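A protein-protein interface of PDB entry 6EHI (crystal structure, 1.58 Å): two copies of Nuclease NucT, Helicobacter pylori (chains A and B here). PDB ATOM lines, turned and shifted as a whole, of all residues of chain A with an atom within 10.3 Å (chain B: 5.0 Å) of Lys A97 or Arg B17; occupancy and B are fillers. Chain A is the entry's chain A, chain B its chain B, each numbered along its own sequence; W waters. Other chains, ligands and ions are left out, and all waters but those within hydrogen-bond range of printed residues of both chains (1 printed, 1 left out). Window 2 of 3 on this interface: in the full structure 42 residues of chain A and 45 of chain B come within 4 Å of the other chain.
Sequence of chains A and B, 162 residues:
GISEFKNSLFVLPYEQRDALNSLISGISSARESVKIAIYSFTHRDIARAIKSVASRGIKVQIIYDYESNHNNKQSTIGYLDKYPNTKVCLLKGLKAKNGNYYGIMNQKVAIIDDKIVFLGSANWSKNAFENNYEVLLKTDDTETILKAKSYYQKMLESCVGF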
ATOM      1  N   GLY A  93       8.736 -12.978  31.655  1.00  0.00           N
ATOM      2  CA  GLY A  93       8.781 -14.374  31.337  1.00  0.00           C
ATOM      3  C   GLY A  93      10.178 -14.840  30.964  1.00  0.00           C
ATOM      4  O   GLY A  93      11.170 -14.107  31.183  1.00  0.00           O
ATOM      5  N   LEU A  94      10.226 -16.038  30.387  1.00  0.00           N
ATOM      6  CA  LEU A  94      11.469 -16.767  30.037  1.00  0.00           C
ATOM      7  C   LEU A  94      12.015 -16.301  28.710  1.00  0.00           C
ATOM      8  O   LEU A  94      11.332 -15.769  27.852  1.00  0.00           O
ATOM      9  CB  LEU A  94      11.217 -18.299  30.029  1.00  0.00           C
ATOM     10  CG  LEU A  94      10.620 -18.990  31.277  1.00  0.00           C
ATOM     11  CD1 LEU A  94      10.513 -20.480  31.210  1.00  0.00           C
ATOM     12  CD2 LEU A  94      11.347 -18.711  32.587  1.00  0.00           C
ATOM     13  N   LYS A  95      13.333 -16.479  28.519  1.00  0.00           N
ATOM     14  CA  LYS A  95      13.889 -16.221  27.199  1.00  0.00           C
ATOM     15  C   LYS A  95      13.432 -17.262  26.133  1.00  0.00           C
ATOM     16  O   LYS A  95      13.427 -18.472  26.350  1.00  0.00           O
ATOM     17  CB  LYS A  95      15.418 -16.190  27.265  1.00  0.00           C
ATOM     18  CG  LYS A  95      16.097 -15.620  25.986  1.00  0.00           C
ATOM     19  CD  LYS A  95      17.624 -15.852  25.992  1.00  0.00           C
ATOM     20  CE  LYS A  95      18.283 -15.274  24.738  1.00  0.00           C
ATOM     21  NZ  LYS A  95      18.629 -13.846  24.990  1.00  0.00           N
ATOM     22  N   ALA A  96      13.054 -16.751  24.982  1.00  0.00           N
ATOM     23  CA  ALA A  96      12.542 -17.575  23.908  1.00  0.00           C
ATOM     24  C   ALA A  96      13.675 -18.468  23.408  1.00  0.00           C
ATOM     25  O   ALA A  96      14.823 -17.992  23.307  1.00  0.00           O
ATOM     26  CB  ALA A  96      12.021 -16.685  22.811  1.00  0.00           C
ATOM     27  N   LYS A  97      13.367 -19.733  23.082  1.00  0.00           N
ATOM     28  CA  LYS A  97      14.440 -20.699  22.686  1.00  0.00           C
ATOM     29  C   LYS A  97      15.171 -20.238  21.430  1.00  0.00           C
ATOM     30  O   LYS A  97      16.381 -20.416  21.297  1.00  0.00           O
ATOM     31  CB  LYS A  97      13.915 -22.125  22.446  1.00  0.00           C
ATOM     32  CG  LYS A  97      13.340 -22.774  23.673  1.00  0.00           C
ATOM     33  CD  LYS A  97      12.757 -24.137  23.344  1.00  0.00           C
ATOM     34  CE  LYS A  97      11.290 -24.276  23.753  1.00  0.00           C
ATOM     35  NZ  LYS A  97      10.586 -25.266  22.882  1.00  0.00           N
ATOM     36  N   ASN A  98      14.460 -19.609  20.504  1.00  0.00           N
ATOM     37  CA  ASN A  98      15.096 -19.259  19.221  1.00  0.00           C
ATOM     38  C   ASN A  98      15.012 -17.743  18.944  1.00  0.00           C
ATOM     39  O   ASN A  98      15.144 -17.297  17.805  1.00  0.00           O
ATOM     40  CB  ASN A  98      14.467 -20.093  18.066  1.00  0.00           C
ATOM     41  CG  ASN A  98      14.748 -21.603  18.152  1.00  0.00           C
ATOM     42  OD1 ASN A  98      15.874 -22.059  18.413  1.00  0.00           O
ATOM     43  ND2 ASN A  98      13.720 -22.383  17.863  1.00  0.00           N
ATOM     44  N   GLY A  99      14.817 -16.943  19.977  1.00  0.00           N
ATOM     45  CA  GLY A  99      14.653 -15.505  19.812  1.00  0.00           C
ATOM     46  C   GLY A  99      15.391 -14.744  20.886  1.00  0.00           C
ATOM     47  O   GLY A  99      15.721 -15.286  21.930  1.00  0.00           O
ATOM     48  N   ASN A 100      15.640 -13.466  20.610  1.00  0.00           N
ATOM     49  CA  ASN A 100      16.237 -12.598  21.584  1.00  0.00           C
ATOM     50  C   ASN A 100      15.168 -11.731  22.245  1.00  0.00           C
ATOM     51  O   ASN A 100      15.281 -10.538  22.347  1.00  0.00           O
ATOM     52  CB  ASN A 100      17.366 -11.776  20.934  1.00  0.00           C
ATOM     53  CG  ASN A 100      18.361 -12.660  20.154  1.00  0.00           C
ATOM     54  OD1 ASN A 100      18.585 -13.840  20.495  1.00  0.00           O
ATOM     55  ND2 ASN A 100      18.946 -12.097  19.098  1.00  0.00           N
ATOM     56  N   TYR A 101      14.146 -12.381  22.764  1.00  0.00           N
ATOM     57  CA  TYR A 101      13.128 -11.699  23.535  1.00  0.00           C
ATOM     58  C   TYR A 101      12.709 -12.585  24.697  1.00  0.00           C
ATOM     59  O   TYR A 101      13.033 -13.771  24.760  1.00  0.00           O
ATOM     60  CB  TYR A 101      11.926 -11.286  22.627  1.00  0.00           C
ATOM     61  CG  TYR A 101      11.127 -12.485  22.089  1.00  0.00           C
ATOM     62  CD1 TYR A 101      11.508 -13.130  20.943  1.00  0.00           C
ATOM     63  CD2 TYR A 101      10.005 -12.991  22.789  1.00  0.00           C
ATOM     64  CE1 TYR A 101      10.797 -14.229  20.470  1.00  0.00           C
ATOM     65  CE2 TYR A 101       9.274 -14.073  22.311  1.00  0.00           C
ATOM     66  CZ  TYR A 101       9.680 -14.696  21.149  1.00  0.00           C
ATOM     67  OH  TYR A 101       9.009 -15.798  20.652  1.00  0.00           O
ATOM     68  N   TYR A 102      12.037 -11.947  25.662  1.00  0.00           N
ATOM     69  CA  TYR A 102      11.474 -12.709  26.795  1.00  0.00           C
ATOM     70  C   TYR A 102       9.908 -12.747  26.737  1.00  0.00           C
ATOM     71  O   TYR A 102       9.299 -11.861  26.180  1.00  0.00           O
ATOM     72  CB  TYR A 102      11.866 -12.096  28.136  1.00  0.00           C
ATOM     73  CG  TYR A 102      13.354 -12.240  28.454  1.00  0.00           C
ATOM     74  CD1 TYR A 102      14.256 -11.292  27.966  1.00  0.00           C
ATOM     75  CD2 TYR A 102      13.841 -13.278  29.207  1.00  0.00           C
ATOM     76  CE1 TYR A 102      15.609 -11.385  28.255  1.00  0.00           C
ATOM     77  CE2 TYR A 102      15.192 -13.390  29.495  1.00  0.00           C
ATOM     78  CZ  TYR A 102      16.064 -12.439  29.016  1.00  0.00           C
ATOM     79  OH  TYR A 102      17.445 -12.531  29.313  1.00  0.00           O
ATOM     80  N   GLY A 103       9.371 -13.792  27.369  1.00  0.00           N
ATOM     81  CA  GLY A 103       7.956 -13.917  27.618  1.00  0.00           C
ATOM     82  C   GLY A 103       7.398 -12.843  28.546  1.00  0.00           C
ATOM     83  O   GLY A 103       8.076 -11.935  29.041  1.00  0.00           O
ATOM     84  N   GLU B  15       4.609 -26.019  34.587  1.00  0.00           N
ATOM     85  CA  GLU B  15       3.853 -27.157  34.067  1.00  0.00           C
ATOM     86  C   GLU B  15       3.474 -27.021  32.559  1.00  0.00           C
ATOM     87  O   GLU B  15       2.500 -27.585  32.131  1.00  0.00           O
ATOM     88  CB  GLU B  15       2.607 -27.324  34.918  1.00  0.00           C
ATOM     89  CG  GLU B  15       2.873 -27.672  36.388  1.00  0.00           C
ATOM     90  CD  GLU B  15       1.574 -27.946  37.058  1.00  0.00           C
ATOM     91  OE1 GLU B  15       0.909 -26.986  37.492  1.00  0.00           O
ATOM     92  OE2 GLU B  15       1.137 -29.086  37.108  1.00  0.00           O
ATOM     93  N   GLN B  16       4.264 -26.322  31.778  1.00  0.00           N
ATOM     94  CA  GLN B  16       3.853 -25.961  30.383  1.00  0.00           C
ATOM     95  C   GLN B  16       3.725 -27.172  29.391  1.00  0.00           C
ATOM     96  O   GLN B  16       2.760 -27.256  28.654  1.00  0.00           O
ATOM     97  CB  GLN B  16       4.756 -24.879  29.826  1.00  0.00           C
ATOM     98  CG  GLN B  16       6.168 -25.339  29.530  1.00  0.00           C
ATOM     99  CD  GLN B  16       7.225 -24.276  29.349  1.00  0.00           C
ATOM    100  OE1 GLN B  16       7.027 -23.079  29.504  1.00  0.00           O
ATOM    101  NE2 GLN B  16       8.427 -24.767  29.002  1.00  0.00           N
ATOM    102  N   ARG B  17       4.626 -28.126  29.558  1.00  0.00           N
ATOM    103  CA  ARG B  17       4.573 -29.419  28.821  1.00  0.00           C
ATOM    104  C   ARG B  17       3.297 -30.177  29.177  1.00  0.00           C
ATOM    105  O   ARG B  17       2.564 -30.622  28.246  1.00  0.00           O
ATOM    106  CB  ARG B  17       5.801 -30.270  29.102  1.00  0.00           C
ATOM    107  CG  ARG B  17       7.153 -29.697  28.642  1.00  0.00           C
ATOM    108  CD  ARG B  17       7.287 -29.579  27.119  1.00  0.00           C
ATOM    109  NE  ARG B  17       8.546 -28.954  26.666  1.00  0.00           N
ATOM    110  CZ  ARG B  17       8.757 -27.652  26.392  1.00  0.00           C
ATOM    111  NH1 ARG B  17       7.807 -26.720  26.536  1.00  0.00           N
ATOM    112  NH2 ARG B  17       9.970 -27.259  25.988  1.00  0.00           N
ATOM    113  N   ASP B  18       2.983 -30.314  30.479  1.00  0.00           N
ATOM    114  CA  ASP B  18       1.807 -31.050  30.891  1.00  0.00           C
ATOM    115  C   ASP B  18       0.524 -30.343  30.481  1.00  0.00           C
ATOM    116  O   ASP B  18      -0.473 -30.988  30.146  1.00  0.00           O
ATOM    117  CB  ASP B  18       1.801 -31.265  32.391  1.00  0.00           C
ATOM    118  CG  ASP B  18       2.701 -32.400  32.807  1.00  0.00           C
ATOM    119  OD1 ASP B  18       3.175 -33.127  31.908  1.00  0.00           O
ATOM    120  OD2 ASP B  18       2.902 -32.536  34.036  1.00  0.00           O
ATOM    121  N   ALA B  19       0.569 -29.011  30.545  1.00  0.00           N
ATOM    122  CA  ALA B  19      -0.600 -28.205  30.175  1.00  0.00           C
ATOM    123  C   ALA B  19      -0.942 -28.381  28.666  1.00  0.00           C
ATOM    124  O   ALA B  19      -2.099 -28.597  28.287  1.00  0.00           O
ATOM    125  CB  ALA B  19      -0.351 -26.783  30.513  1.00  0.00           C
ATOM    126  N   LEU B  20       0.067 -28.284  27.819  1.00  0.00           N
ATOM    127  CA  LEU B  20      -0.146 -28.419  26.376  1.00  0.00           C
ATOM    128  C   LEU B  20      -0.609 -29.823  26.083  1.00  0.00           C
ATOM    129  O   LEU B  20      -1.540 -30.074  25.270  1.00  0.00           O
ATOM    130  CB  LEU B  20       1.148 -28.104  25.608  1.00  0.00           C
ATOM    131  CG  LEU B  20       1.032 -28.256  24.114  1.00  0.00           C
ATOM    132  CD1 LEU B  20       0.055 -27.225  23.611  1.00  0.00           C
ATOM    133  CD2 LEU B  20       2.401 -28.030  23.516  1.00  0.00           C
ATOM    134  N   ASN B  21       0.029 -30.784  26.708  1.00  0.00           N
ATOM    135  CA  ASN B  21      -0.378 -32.204  26.528  1.00  0.00           C
ATOM    136  C   ASN B  21      -1.823 -32.398  26.937  1.00  0.00           C
ATOM    137  O   ASN B  21      -2.573 -33.058  26.222  1.00  0.00           O
ATOM    138  CB  ASN B  21       0.556 -33.111  27.301  1.00  0.00           C
ATOM    139  CG  ASN B  21       1.944 -33.243  26.641  1.00  0.00           C
ATOM    140  OD1 ASN B  21       2.114 -32.944  25.457  1.00  0.00           O
ATOM    141  ND2 ASN B  21       2.961 -33.654  27.441  1.00  0.00           N
ATOM    142  N   SER B  22      -2.273 -31.782  28.040  1.00  0.00           N
ATOM    143  CA  SER B  22      -3.616 -31.931  28.526  1.00  0.00           C
ATOM    144  C   SER B  22      -4.620 -31.332  27.546  1.00  0.00           C
ATOM    145  O   SER B  22      -5.692 -31.959  27.262  1.00  0.00           O
ATOM    146  CB  SER B  22      -3.781 -31.313  29.934  1.00  0.00           C
ATOM    147  OG  SER B  22      -5.119 -31.342  30.299  1.00  0.00           O
ATOM    148  N   PHE B 129       2.940 -21.357  25.685  1.00  0.00           N
ATOM    149  CA  PHE B 129       3.273 -22.652  26.203  1.00  0.00           C
ATOM    150  C   PHE B 129       4.817 -22.861  26.328  1.00  0.00           C
ATOM    151  O   PHE B 129       5.240 -23.928  26.729  1.00  0.00           O
ATOM    152  CB  PHE B 129       2.646 -23.722  25.363  1.00  0.00           C
ATOM    153  CG  PHE B 129       1.223 -23.847  25.590  1.00  0.00           C
ATOM    154  CD1 PHE B 129       0.762 -24.688  26.581  1.00  0.00           C
ATOM    155  CD2 PHE B 129       0.305 -23.131  24.829  1.00  0.00           C
ATOM    156  CE1 PHE B 129      -0.548 -24.817  26.815  1.00  0.00           C
ATOM    157  CE2 PHE B 129      -1.055 -23.218  25.036  1.00  0.00           C
ATOM    158  CZ  PHE B 129      -1.512 -24.011  26.045  1.00  0.00           C
ATOM    159  N   GLU B 130       5.600 -21.873  25.958  1.00  0.00           N
ATOM    160  CA  GLU B 130       7.048 -21.944  26.170  1.00  0.00           C
ATOM    161  C   GLU B 130       7.642 -20.872  27.007  1.00  0.00           C
ATOM    162  O   GLU B 130       8.623 -21.148  27.676  1.00  0.00           O
ATOM    163  CB  GLU B 130       7.755 -21.846  24.806  1.00  0.00           C
ATOM    164  CG  GLU B 130       7.365 -23.045  23.989  1.00  0.00           C
ATOM    165  CD  GLU B 130       8.013 -23.110  22.638  1.00  0.00           C
ATOM    166  OE1 GLU B 130       8.800 -22.191  22.224  1.00  0.00           O
ATOM    167  OE2 GLU B 130       7.611 -24.077  21.940  1.00  0.00           O
ATOM    168  N   ASN B 131       7.190 -19.612  26.860  1.00  0.00           N
ATOM    169  CA  ASN B 131       7.877 -18.503  27.496  1.00  0.00           C
ATOM    170  C   ASN B 131       7.190 -17.760  28.612  1.00  0.00           C
ATOM    171  O   ASN B 131       7.798 -16.968  29.276  1.00  0.00           O
ATOM    172  CB  ASN B 131       8.277 -17.478  26.441  1.00  0.00           C
ATOM    173  CG  ASN B 131       8.995 -18.107  25.263  1.00  0.00           C
ATOM    174  OD1 ASN B 131       9.812 -19.047  25.418  1.00  0.00           O
ATOM    175  ND2 ASN B 131       8.654 -17.654  24.096  1.00  0.00           N
HETATM  176  O   HOH W   1      10.698 -20.738  23.489  1.00  0.00           O
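The backbone NH (N) of Leu A94 sits at hydrogen-bond distance from the backbone carbonyl oxygen (O) of Asn B131. The side-chain amino group (NZ) of Lys A97 lies within salt-bridge range of the side-chain carboxylate (OE2) of Glu B130, 3.3 Å away.
The backbone NH (N) of Gly A93 lies within hydrogen-bond range of the backbone carbonyl oxygen (O) of Gly A103 (2.9 Å). N of Gly A103 lies within hydrogen-bond range of O of Leu A94. O of Tyr A101 is in hydrogen-bond range of N of Ala A96, at 3.0 Å. NH1 of Arg B17 lies close to NE2 of Gln B16. The side-chain amide oxygen (OE1) of Gln B16 lies close to the backbone carbonyl oxygen (O) of Glu B130 (3.1 Å). ND2 of Asn B21 sits close to O of Arg B17, 3.2 Å away.
Gly A93 touches Asn B131. Lys A95 touches Asn B131 (O to OD1, 3.8 Å). Ala A96 touches Asn B131 (CA to OD1, 3.4 Å). NH2 of Arg B17 touches NZ of Lys A97, at 3.7 Å. Tyr A101 touches Asn B131 (OH to ND2, 3.9 Å). Gly A103 touches Asn B131 (CA to O, 3.5 Å).
Lys A97 touches just these residues of chain B: Arg B17 (3.7 Å) and Glu B130 (3.3 Å). Of chain A, only Lys A97 (3.7 Å) comes within 4 Å of Arg B17. Gln B16 touches none of the printed residues of chain A. No residue of chain A comes within 4 Å of Asn B21. Of the printed residues of chain B, Lys A95 touches Asn B131. Of the printed residues of chain B, Gly A93 touches Asn B131. Gly A99 touches none of the printed residues of chain B. Phe B129 touches none of the printed residues of chain A. The nearest residue of chain B that does not touch Lys A97 is Asn B131 (4.3 Å). The nearest residue of chain A that does not touch Arg B17 is Leu A94 (8.3 Å). The nearest printed residue of chain B that does not touch Leu A94 is Glu B130 (4.1 Å).
Of the 11 printed residues of chain A, 7 touch a printed residue of chain B. Hydrophobic or aromatic side chains of chain A that line the printed part of chain B: Leu A94, Ala A96 and Tyr A101. Among the printed residues, Asp or Glu carboxylates within 4 Å of a Lys or Arg side-chain nitrogen of the other chain: Lys A97 with Glu B130.
No position is printed for both chains. Of the 8 pairs that touch across the chains among the printed residues, none has its exchanged pair printed and touching as well.
Water W1 lies within hydrogen-bond range of the side-chain carboxylate of Glu B130 (2.7 Å), the side-chain amide oxygen of Asn B131 (2.7 Å) and the backbone NH of Lys A97 (2.9 Å).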
